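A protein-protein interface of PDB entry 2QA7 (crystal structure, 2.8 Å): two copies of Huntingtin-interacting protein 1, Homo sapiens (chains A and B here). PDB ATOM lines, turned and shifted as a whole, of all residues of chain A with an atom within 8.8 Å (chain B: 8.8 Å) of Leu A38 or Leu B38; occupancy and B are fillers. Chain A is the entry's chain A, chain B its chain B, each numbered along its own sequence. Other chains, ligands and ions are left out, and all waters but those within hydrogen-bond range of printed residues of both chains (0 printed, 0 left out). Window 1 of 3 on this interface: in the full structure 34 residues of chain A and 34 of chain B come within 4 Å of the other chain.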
ATOM      1  N   SER A  31      16.187 -15.323 -30.106  1.00  0.00           N
ATOM      2  CA  SER A  31      17.461 -16.013 -30.136  1.00  0.00           C
ATOM      3  C   SER A  31      18.498 -15.173 -30.885  1.00  0.00           C
ATOM      4  O   SER A  31      19.602 -14.975 -30.391  1.00  0.00           O
ATOM      5  CB  SER A  31      17.307 -17.389 -30.788  1.00  0.00           C
ATOM      6  OG  SER A  31      18.527 -18.113 -30.746  1.00  0.00           O
ATOM      7  N   GLN A  32      18.147 -14.669 -32.066  1.00  0.00           N
ATOM      8  CA  GLN A  32      19.074 -13.846 -32.842  1.00  0.00           C
ATOM      9  C   GLN A  32      19.593 -12.682 -32.002  1.00  0.00           C
ATOM     10  O   GLN A  32      20.799 -12.459 -31.913  1.00  0.00           O
ATOM     11  CB  GLN A  32      18.387 -13.271 -34.089  1.00  0.00           C
ATOM     12  CG  GLN A  32      17.828 -14.301 -35.047  1.00  0.00           C
ATOM     13  CD  GLN A  32      18.888 -15.248 -35.556  1.00  0.00           C
ATOM     14  OE1 GLN A  32      19.833 -14.831 -36.226  1.00  0.00           O
ATOM     15  NE2 GLN A  32      18.741 -16.533 -35.237  1.00  0.00           N
ATOM     16  N   ARG A  33      18.672 -11.941 -31.392  1.00  0.00           N
ATOM     17  CA  ARG A  33      19.033 -10.788 -30.579  1.00  0.00           C
ATOM     18  C   ARG A  33      19.955 -11.179 -29.438  1.00  0.00           C
ATOM     19  O   ARG A  33      21.079 -10.695 -29.342  1.00  0.00           O
ATOM     20  CB  ARG A  33      17.772 -10.096 -30.039  1.00  0.00           C
ATOM     21  CG  ARG A  33      16.800  -9.643 -31.144  1.00  0.00           C
ATOM     22  CD  ARG A  33      15.738  -8.661 -30.631  1.00  0.00           C
ATOM     23  NE  ARG A  33      14.752  -8.281 -31.651  1.00  0.00           N
ATOM     24  CZ  ARG A  33      15.046  -7.746 -32.835  1.00  0.00           C
ATOM     25  NH1 ARG A  33      16.308  -7.517 -33.175  1.00  0.00           N
ATOM     26  NH2 ARG A  33      14.074  -7.429 -33.681  1.00  0.00           N
ATOM     27  N   VAL A  34      19.478 -12.061 -28.573  1.00  0.00           N
ATOM     28  CA  VAL A  34      20.264 -12.532 -27.441  1.00  0.00           C
ATOM     29  C   VAL A  34      21.690 -12.984 -27.850  1.00  0.00           C
ATOM     30  O   VAL A  34      22.684 -12.497 -27.313  1.00  0.00           O
ATOM     31  CB  VAL A  34      19.500 -13.682 -26.741  1.00  0.00           C
ATOM     32  CG1 VAL A  34      20.376 -14.390 -25.734  1.00  0.00           C
ATOM     33  CG2 VAL A  34      18.272 -13.121 -26.065  1.00  0.00           C
ATOM     34  N   VAL A  35      21.796 -13.900 -28.806  1.00  0.00           N
ATOM     35  CA  VAL A  35      23.100 -14.373 -29.239  1.00  0.00           C
ATOM     36  C   VAL A  35      23.996 -13.236 -29.709  1.00  0.00           C
ATOM     37  O   VAL A  35      25.184 -13.207 -29.393  1.00  0.00           O
ATOM     38  CB  VAL A  35      22.985 -15.401 -30.380  1.00  0.00           C
ATOM     39  CG1 VAL A  35      24.364 -15.747 -30.908  1.00  0.00           C
ATOM     40  CG2 VAL A  35      22.316 -16.653 -29.880  1.00  0.00           C
ATOM     41  N   LEU A  36      23.438 -12.304 -30.469  1.00  0.00           N
ATOM     42  CA  LEU A  36      24.234 -11.187 -30.959  1.00  0.00           C
ATOM     43  C   LEU A  36      24.724 -10.311 -29.820  1.00  0.00           C
ATOM     44  O   LEU A  36      25.895  -9.974 -29.749  1.00  0.00           O
ATOM     45  CB  LEU A  36      23.432 -10.333 -31.943  1.00  0.00           C
ATOM     46  CG  LEU A  36      23.109 -10.946 -33.302  1.00  0.00           C
ATOM     47  CD1 LEU A  36      22.494  -9.882 -34.183  1.00  0.00           C
ATOM     48  CD2 LEU A  36      24.368 -11.494 -33.946  1.00  0.00           C
ATOM     49  N   GLN A  37      23.824  -9.939 -28.925  1.00  0.00           N
ATOM     50  CA  GLN A  37      24.204  -9.105 -27.807  1.00  0.00           C
ATOM     51  C   GLN A  37      25.367  -9.730 -27.037  1.00  0.00           C
ATOM     52  O   GLN A  37      26.345  -9.050 -26.710  1.00  0.00           O
ATOM     53  CB  GLN A  37      23.007  -8.898 -26.892  1.00  0.00           C
ATOM     54  CG  GLN A  37      23.226  -7.859 -25.829  1.00  0.00           C
ATOM     55  CD  GLN A  37      21.953  -7.552 -25.076  1.00  0.00           C
ATOM     56  OE1 GLN A  37      20.926  -7.233 -25.682  1.00  0.00           O
ATOM     57  NE2 GLN A  37      22.009  -7.646 -23.749  1.00  0.00           N
ATOM     58  N   LEU A  38      25.270 -11.026 -26.753  1.00  0.00           N
ATOM     59  CA  LEU A  38      26.332 -11.707 -26.022  1.00  0.00           C
ATOM     60  C   LEU A  38      27.632 -11.663 -26.808  1.00  0.00           C
ATOM     61  O   LEU A  38      28.682 -11.314 -26.269  1.00  0.00           O
ATOM     62  CB  LEU A  38      25.949 -13.159 -25.724  1.00  0.00           C
ATOM     63  CG  LEU A  38      25.073 -13.381 -24.489  1.00  0.00           C
ATOM     64  CD1 LEU A  38      24.715 -14.843 -24.383  1.00  0.00           C
ATOM     65  CD2 LEU A  38      25.805 -12.935 -23.242  1.00  0.00           C
ATOM     66  N   LYS A  39      27.565 -12.003 -28.088  1.00  0.00           N
ATOM     67  CA  LYS A  39      28.758 -11.971 -28.917  1.00  0.00           C
ATOM     68  C   LYS A  39      29.487 -10.621 -28.840  1.00  0.00           C
ATOM     69  O   LYS A  39      30.709 -10.561 -28.926  1.00  0.00           O
ATOM     70  CB  LYS A  39      28.405 -12.300 -30.370  1.00  0.00           C
ATOM     71  CG  LYS A  39      28.031 -13.752 -30.586  1.00  0.00           C
ATOM     72  CD  LYS A  39      28.208 -14.167 -32.035  1.00  0.00           C
ATOM     73  CE  LYS A  39      27.988 -15.670 -32.194  1.00  0.00           C
ATOM     74  NZ  LYS A  39      28.309 -16.179 -33.566  1.00  0.00           N
ATOM     75  N   GLY A  40      28.738  -9.541 -28.668  1.00  0.00           N
ATOM     76  CA  GLY A  40      29.354  -8.235 -28.587  1.00  0.00           C
ATOM     77  C   GLY A  40      29.908  -7.997 -27.209  1.00  0.00           C
ATOM     78  O   GLY A  40      30.919  -7.326 -27.023  1.00  0.00           O
ATOM     79  N   HIS A  41      29.227  -8.552 -26.223  1.00  0.00           N
ATOM     80  CA  HIS A  41      29.671  -8.409 -24.858  1.00  0.00           C
ATOM     81  C   HIS A  41      31.073  -9.035 -24.821  1.00  0.00           C
ATOM     82  O   HIS A  41      32.015  -8.471 -24.265  1.00  0.00           O
ATOM     83  CB  HIS A  41      28.686  -9.145 -23.951  1.00  0.00           C
ATOM     84  CG  HIS A  41      28.792  -8.777 -22.505  1.00  0.00           C
ATOM     85  ND1 HIS A  41      27.775  -9.014 -21.607  1.00  0.00           N
ATOM     86  CD2 HIS A  41      29.807  -8.238 -21.789  1.00  0.00           C
ATOM     87  CE1 HIS A  41      28.159  -8.641 -20.400  1.00  0.00           C
ATOM     88  NE2 HIS A  41      29.389  -8.168 -20.483  1.00  0.00           N
ATOM     89  N   VAL A  42      31.209 -10.193 -25.452  1.00  0.00           N
ATOM     90  CA  VAL A  42      32.489 -10.882 -25.485  1.00  0.00           C
ATOM     91  C   VAL A  42      33.563  -9.988 -26.064  1.00  0.00           C
ATOM     92  O   VAL A  42      34.636  -9.866 -25.495  1.00  0.00           O
ATOM     93  CB  VAL A  42      32.421 -12.159 -26.333  1.00  0.00           C
ATOM     94  CG1 VAL A  42      33.811 -12.761 -26.472  1.00  0.00           C
ATOM     95  CG2 VAL A  42      31.472 -13.154 -25.686  1.00  0.00           C
ATOM     96  N   SER A  43      33.269  -9.370 -27.205  1.00  0.00           N
ATOM     97  CA  SER A  43      34.215  -8.480 -27.874  1.00  0.00           C
ATOM     98  C   SER A  43      34.586  -7.325 -26.980  1.00  0.00           C
ATOM     99  O   SER A  43      35.751  -6.967 -26.906  1.00  0.00           O
ATOM    100  CB  SER A  43      33.631  -7.938 -29.176  1.00  0.00           C
ATOM    101  OG  SER A  43      33.500  -8.975 -30.133  1.00  0.00           O
ATOM    102  N   GLU A  44      33.598  -6.735 -26.308  1.00  0.00           N
ATOM    103  CA  GLU A  44      33.880  -5.627 -25.410  1.00  0.00           C
ATOM    104  C   GLU A  44      34.832  -6.076 -24.294  1.00  0.00           C
ATOM    105  O   GLU A  44      35.660  -5.310 -23.814  1.00  0.00           O
ATOM    106  CB  GLU A  44      32.581  -5.068 -24.828  1.00  0.00           C
ATOM    107  CG  GLU A  44      31.798  -4.176 -25.797  1.00  0.00           C
ATOM    108  CD  GLU A  44      32.651  -3.061 -26.397  1.00  0.00           C
ATOM    109  OE1 GLU A  44      33.266  -2.297 -25.627  1.00  0.00           O
ATOM    110  OE2 GLU A  44      32.709  -2.945 -27.640  1.00  0.00           O
ATOM    111  N   LEU A  45      34.717  -7.331 -23.889  1.00  0.00           N
ATOM    112  CA  LEU A  45      35.586  -7.852 -22.859  1.00  0.00           C
ATOM    113  C   LEU A  45      36.866  -8.351 -23.521  1.00  0.00           C
ATOM    114  O   LEU A  45      37.951  -8.056 -23.027  1.00  0.00           O
ATOM    115  CB  LEU A  45      34.879  -8.975 -22.110  1.00  0.00           C
ATOM    116  CG  LEU A  45      33.551  -8.533 -21.499  1.00  0.00           C
ATOM    117  CD1 LEU A  45      32.875  -9.688 -20.804  1.00  0.00           C
ATOM    118  CD2 LEU A  45      33.814  -7.437 -20.508  1.00  0.00           C
ATOM    119  N   GLU A  46      36.732  -9.097 -24.629  1.00  0.00           N
ATOM    120  CA  GLU A  46      37.885  -9.618 -25.390  1.00  0.00           C
ATOM    121  C   GLU A  46      38.862  -8.378 -25.345  1.00  0.00           C
ATOM    122  O   GLU A  46      40.073  -8.539 -25.164  1.00  0.00           O
ATOM    123  CB  GLU A  46      37.463 -10.034 -26.884  1.00  0.00           C
ATOM    124  CG  GLU A  46      37.621 -11.586 -27.428  1.00  0.00           C
ATOM    125  CD  GLU A  46      37.162 -11.914 -28.978  1.00  0.00           C
ATOM    126  OE1 GLU A  46      37.747 -11.516 -30.016  1.00  0.00           O
ATOM    127  OE2 GLU A  46      36.183 -12.648 -29.187  1.00  0.00           O
ATOM    128  N   SER B  31      19.370 -23.175 -29.425  1.00  0.00           N
ATOM    129  CA  SER B  31      19.533 -21.840 -28.878  1.00  0.00           C
ATOM    130  C   SER B  31      20.183 -21.905 -27.493  1.00  0.00           C
ATOM    131  O   SER B  31      21.034 -21.085 -27.151  1.00  0.00           O
ATOM    132  CB  SER B  31      18.165 -21.159 -28.795  1.00  0.00           C
ATOM    133  OG  SER B  31      18.266 -19.804 -28.405  1.00  0.00           O
ATOM    134  N   GLN B  32      19.788 -22.888 -26.695  1.00  0.00           N
ATOM    135  CA  GLN B  32      20.339 -23.025 -25.354  1.00  0.00           C
ATOM    136  C   GLN B  32      21.771 -23.532 -25.366  1.00  0.00           C
ATOM    137  O   GLN B  32      22.579 -23.135 -24.532  1.00  0.00           O
ATOM    138  CB  GLN B  32      19.478 -23.974 -24.512  1.00  0.00           C
ATOM    139  CG  GLN B  32      18.135 -23.398 -24.088  1.00  0.00           C
ATOM    140  CD  GLN B  32      17.176 -24.443 -23.526  1.00  0.00           C
ATOM    141  OE1 GLN B  32      16.086 -24.103 -23.075  1.00  0.00           O
ATOM    142  NE2 GLN B  32      17.576 -25.717 -23.562  1.00  0.00           N
ATOM    143  N   ARG B  33      22.088 -24.410 -26.306  1.00  0.00           N
ATOM    144  CA  ARG B  33      23.428 -24.965 -26.376  1.00  0.00           C
ATOM    145  C   ARG B  33      24.411 -23.849 -26.664  1.00  0.00           C
ATOM    146  O   ARG B  33      25.581 -23.911 -26.269  1.00  0.00           O
ATOM    147  CB  ARG B  33      23.506 -26.031 -27.468  1.00  0.00           C
ATOM    148  CG  ARG B  33      24.751 -26.904 -27.385  1.00  0.00           C
ATOM    149  CD  ARG B  33      25.719 -26.563 -28.485  1.00  0.00           C
ATOM    150  NE  ARG B  33      25.212 -26.970 -29.788  1.00  0.00           N
ATOM    151  CZ  ARG B  33      25.677 -26.501 -30.937  1.00  0.00           C
ATOM    152  NH1 ARG B  33      26.655 -25.607 -30.940  1.00  0.00           N
ATOM    153  NH2 ARG B  33      25.170 -26.930 -32.083  1.00  0.00           N
ATOM    154  N   VAL B  34      23.919 -22.815 -27.335  1.00  0.00           N
ATOM    155  CA  VAL B  34      24.751 -21.678 -27.682  1.00  0.00           C
ATOM    156  C   VAL B  34      24.749 -20.594 -26.617  1.00  0.00           C
ATOM    157  O   VAL B  34      25.806 -20.150 -26.186  1.00  0.00           O
ATOM    158  CB  VAL B  34      24.310 -21.057 -29.018  1.00  0.00           C
ATOM    159  CG1 VAL B  34      25.220 -19.921 -29.382  1.00  0.00           C
ATOM    160  CG2 VAL B  34      24.336 -22.107 -30.105  1.00  0.00           C
ATOM    161  N   VAL B  35      23.574 -20.166 -26.182  1.00  0.00           N
ATOM    162  CA  VAL B  35      23.530 -19.115 -25.183  1.00  0.00           C
ATOM    163  C   VAL B  35      24.278 -19.478 -23.918  1.00  0.00           C
ATOM    164  O   VAL B  35      24.783 -18.603 -23.213  1.00  0.00           O
ATOM    165  CB  VAL B  35      22.107 -18.731 -24.845  1.00  0.00           C
ATOM    166  CG1 VAL B  35      22.096 -17.833 -23.637  1.00  0.00           C
ATOM    167  CG2 VAL B  35      21.509 -17.981 -26.018  1.00  0.00           C
ATOM    168  N   LEU B  36      24.351 -20.769 -23.622  1.00  0.00           N
ATOM    169  CA  LEU B  36      25.080 -21.207 -22.446  1.00  0.00           C
ATOM    170  C   LEU B  36      26.566 -21.049 -22.732  1.00  0.00           C
ATOM    171  O   LEU B  36      27.290 -20.449 -21.942  1.00  0.00           O
ATOM    172  CB  LEU B  36      24.760 -22.665 -22.105  1.00  0.00           C
ATOM    173  CG  LEU B  36      23.577 -22.904 -21.160  1.00  0.00           C
ATOM    174  CD1 LEU B  36      23.494 -24.380 -20.795  1.00  0.00           C
ATOM    175  CD2 LEU B  36      23.754 -22.074 -19.899  1.00  0.00           C
ATOM    176  N   GLN B  37      27.012 -21.571 -23.873  1.00  0.00           N
ATOM    177  CA  GLN B  37      28.416 -21.485 -24.259  1.00  0.00           C
ATOM    178  C   GLN B  37      28.892 -20.038 -24.346  1.00  0.00           C
ATOM    179  O   GLN B  37      30.033 -19.739 -24.001  1.00  0.00           O
ATOM    180  CB  GLN B  37      28.638 -22.204 -25.593  1.00  0.00           C
ATOM    181  CG  GLN B  37      30.035 -22.051 -26.184  1.00  0.00           C
ATOM    182  CD  GLN B  37      30.059 -21.125 -27.395  1.00  0.00           C
ATOM    183  OE1 GLN B  37      29.348 -21.353 -28.377  1.00  0.00           O
ATOM    184  NE2 GLN B  37      30.879 -20.077 -27.331  1.00  0.00           N
ATOM    185  N   LEU B  38      28.015 -19.141 -24.792  1.00  0.00           N
ATOM    186  CA  LEU B  38      28.369 -17.729 -24.908  1.00  0.00           C
ATOM    187  C   LEU B  38      28.409 -17.050 -23.544  1.00  0.00           C
ATOM    188  O   LEU B  38      29.250 -16.184 -23.298  1.00  0.00           O
ATOM    189  CB  LEU B  38      27.391 -17.000 -25.838  1.00  0.00           C
ATOM    190  CG  LEU B  38      27.836 -16.913 -27.304  1.00  0.00           C
ATOM    191  CD1 LEU B  38      26.701 -16.443 -28.180  1.00  0.00           C
ATOM    192  CD2 LEU B  38      28.994 -15.953 -27.416  1.00  0.00           C
ATOM    193  N   LYS B  39      27.494 -17.444 -22.664  1.00  0.00           N
ATOM    194  CA  LYS B  39      27.446 -16.896 -21.314  1.00  0.00           C
ATOM    195  C   LYS B  39      28.671 -17.366 -20.534  1.00  0.00           C
ATOM    196  O   LYS B  39      29.249 -16.623 -19.739  1.00  0.00           O
ATOM    197  CB  LYS B  39      26.202 -17.382 -20.584  1.00  0.00           C
ATOM    198  CG  LYS B  39      24.950 -16.610 -20.873  1.00  0.00           C
ATOM    199  CD  LYS B  39      23.872 -17.009 -19.888  1.00  0.00           C
ATOM    200  CE  LYS B  39      22.727 -16.034 -19.925  1.00  0.00           C
ATOM    201  NZ  LYS B  39      22.159 -15.951 -21.290  1.00  0.00           N
ATOM    202  N   GLY B  40      29.056 -18.616 -20.759  1.00  0.00           N
ATOM    203  CA  GLY B  40      30.199 -19.169 -20.067  1.00  0.00           C
ATOM    204  C   GLY B  40      31.455 -18.443 -20.458  1.00  0.00           C
ATOM    205  O   GLY B  40      32.274 -18.075 -19.615  1.00  0.00           O
ATOM    206  N   HIS B  41      31.613 -18.234 -21.754  1.00  0.00           N
ATOM    207  CA  HIS B  41      32.784 -17.538 -22.236  1.00  0.00           C
ATOM    208  C   HIS B  41      32.799 -16.165 -21.599  1.00  0.00           C
ATOM    209  O   HIS B  41      33.849 -15.651 -21.225  1.00  0.00           O
ATOM    210  CB  HIS B  41      32.732 -17.384 -23.742  1.00  0.00           C
ATOM    211  CG  HIS B  41      33.976 -16.799 -24.314  1.00  0.00           C
ATOM    212  ND1 HIS B  41      34.095 -16.450 -25.639  1.00  0.00           N
ATOM    213  CD2 HIS B  41      35.164 -16.507 -23.737  1.00  0.00           C
ATOM    214  CE1 HIS B  41      35.304 -15.966 -25.855  1.00  0.00           C
ATOM    215  NE2 HIS B  41      35.973 -15.989 -24.718  1.00  0.00           N
ATOM    216  N   VAL B  42      31.619 -15.575 -21.474  1.00  0.00           N
ATOM    217  CA  VAL B  42      31.508 -14.258 -20.884  1.00  0.00           C
ATOM    218  C   VAL B  42      31.944 -14.261 -19.432  1.00  0.00           C
ATOM    219  O   VAL B  42      32.718 -13.405 -19.017  1.00  0.00           O
ATOM    220  CB  VAL B  42      30.070 -13.719 -20.990  1.00  0.00           C
ATOM    221  CG1 VAL B  42      29.911 -12.488 -20.143  1.00  0.00           C
ATOM    222  CG2 VAL B  42      29.757 -13.373 -22.432  1.00  0.00           C
ATOM    223  N   SER B  43      31.459 -15.225 -18.658  1.00  0.00           N
ATOM    224  CA  SER B  43      31.821 -15.290 -17.249  1.00  0.00           C
ATOM    225  C   SER B  43      33.320 -15.512 -17.079  1.00  0.00           C
ATOM    226  O   SER B  43      33.924 -14.979 -16.146  1.00  0.00           O
ATOM    227  CB  SER B  43      31.030 -16.388 -16.547  1.00  0.00           C
ATOM    228  OG  SER B  43      31.107 -17.580 -17.296  1.00  0.00           O
ATOM    229  N   GLU B  44      33.924 -16.297 -17.967  1.00  0.00           N
ATOM    230  CA  GLU B  44      35.362 -16.504 -17.890  1.00  0.00           C
ATOM    231  C   GLU B  44      36.021 -15.128 -18.003  1.00  0.00           C
ATOM    232  O   GLU B  44      36.718 -14.677 -17.095  1.00  0.00           O
ATOM    233  CB  GLU B  44      35.851 -17.376 -19.040  1.00  0.00           C
ATOM    234  CG  GLU B  44      35.567 -18.852 -18.895  1.00  0.00           C
ATOM    235  CD  GLU B  44      36.209 -19.655 -20.009  1.00  0.00           C
ATOM    236  OE1 GLU B  44      37.429 -19.489 -20.231  1.00  0.00           O
ATOM    237  OE2 GLU B  44      35.498 -20.448 -20.662  1.00  0.00           O
ATOM    238  N   LEU B  45      35.790 -14.464 -19.132  1.00  0.00           N
ATOM    239  CA  LEU B  45      36.340 -13.143 -19.368  1.00  0.00           C
ATOM    240  C   LEU B  45      36.138 -12.194 -18.179  1.00  0.00           C
ATOM    241  O   LEU B  45      37.089 -11.549 -17.725  1.00  0.00           O
ATOM    242  CB  LEU B  45      35.705 -12.539 -20.617  1.00  0.00           C
ATOM    243  CG  LEU B  45      36.144 -13.140 -21.955  1.00  0.00           C
ATOM    244  CD1 LEU B  45      35.094 -12.849 -23.016  1.00  0.00           C
ATOM    245  CD2 LEU B  45      37.493 -12.568 -22.360  1.00  0.00           C
ATOM    246  N   GLU B  46      34.911 -12.103 -17.672  1.00  0.00           N
ATOM    247  CA  GLU B  46      34.644 -11.210 -16.546  1.00  0.00           C
ATOM    248  C   GLU B  46      35.651 -11.495 -15.441  1.00  0.00           C
ATOM    249  O   GLU B  46      36.251 -10.581 -14.873  1.00  0.00           O
ATOM    250  CB  GLU B  46      33.217 -11.397 -16.018  1.00  0.00           C
ATOM    251  CG  GLU B  46      32.125 -11.346 -17.090  1.00  0.00           C
ATOM    252  CD  GLU B  46      30.965 -10.422 -16.738  1.00  0.00           C
ATOM    253  OE1 GLU B  46      31.102  -9.195 -16.926  1.00  0.00           O
ATOM    254  OE2 GLU B  46      29.916 -10.920 -16.271  1.00  0.00           O
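The side-chain hydroxyl (OG) of Ser A31 lies within hydrogen-bond range of the side-chain hydroxyl (OG) of Ser B31.
Leu A38 touches just these residues of chain B: Val B35, Leu B38 and Lys B39.
Leu B38 touches just these residues of chain A: Val A35, Leu A38 and Lys A39.
Gly A40 touches none of the printed residues of chain B.
No residue of chain A comes within 4 Å of Gln B37.
Of the printed residues of chain B, Leu A45 touches Leu B45 (3.95 Å).
Printed residues of chain B within 4 Å of Val A42: His B41 (3.6 Å), Val B42 (3.7 Å) and Leu B45 (3.7 Å).
Of the printed residues of chain A, Leu B45 touches Val A42 (3.7 Å) and Leu A45 (3.95 Å).
Printed residues of chain B within 4 Å of Val A34: Val B35 (3.8 Å).
Glu B46 touches none of the printed residues of chain A.
Ser A43 touches none of the printed residues of chain B.
The nearest residue of chain B that does not touch Leu A38 is Val B42 (4.1 Å).
The nearest residue of chain A that does not touch Leu B38 is Val A42 (4.1 Å).
The backbone carbonyl oxygen (O) of Lys B39 sits at hydrogen-bond distance from the side-chain hydroxyl (OG) of Ser B43 (3.2 Å).
The side-chain hydroxyl of Ser A43 lies within hydrogen-bond range of the backbone carbonyl oxygen of Lys A39 (3.4 Å).
Ser A31 touches its own counterpart, Ser B31.
Val A35 touches Leu B38, and with the chains exchanged Leu A38 touches Val B35.
Leu A38 touches Lys B39, and with the chains exchanged Lys A39 touches Leu B38.
Val A42 touches His B41, but with the chains exchanged His A41 does not touch Val B42 (4.2 Å).
16 positions are printed for both chains.
Among the printed residues, 11 pairs touch across the chains.
Among the printed residues, pairs that only touch across the chains: Val A34 with Val B35, Val A35 with Leu B38, Leu A38 with Val B35, Leu A38 with Leu B38, Leu A38 with Lys B39, Lys A39 with Leu B38, Val A42 with His B41, Val A42 with Val B42, Val A42 with Leu B45 and Leu A45 with Leu B45.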
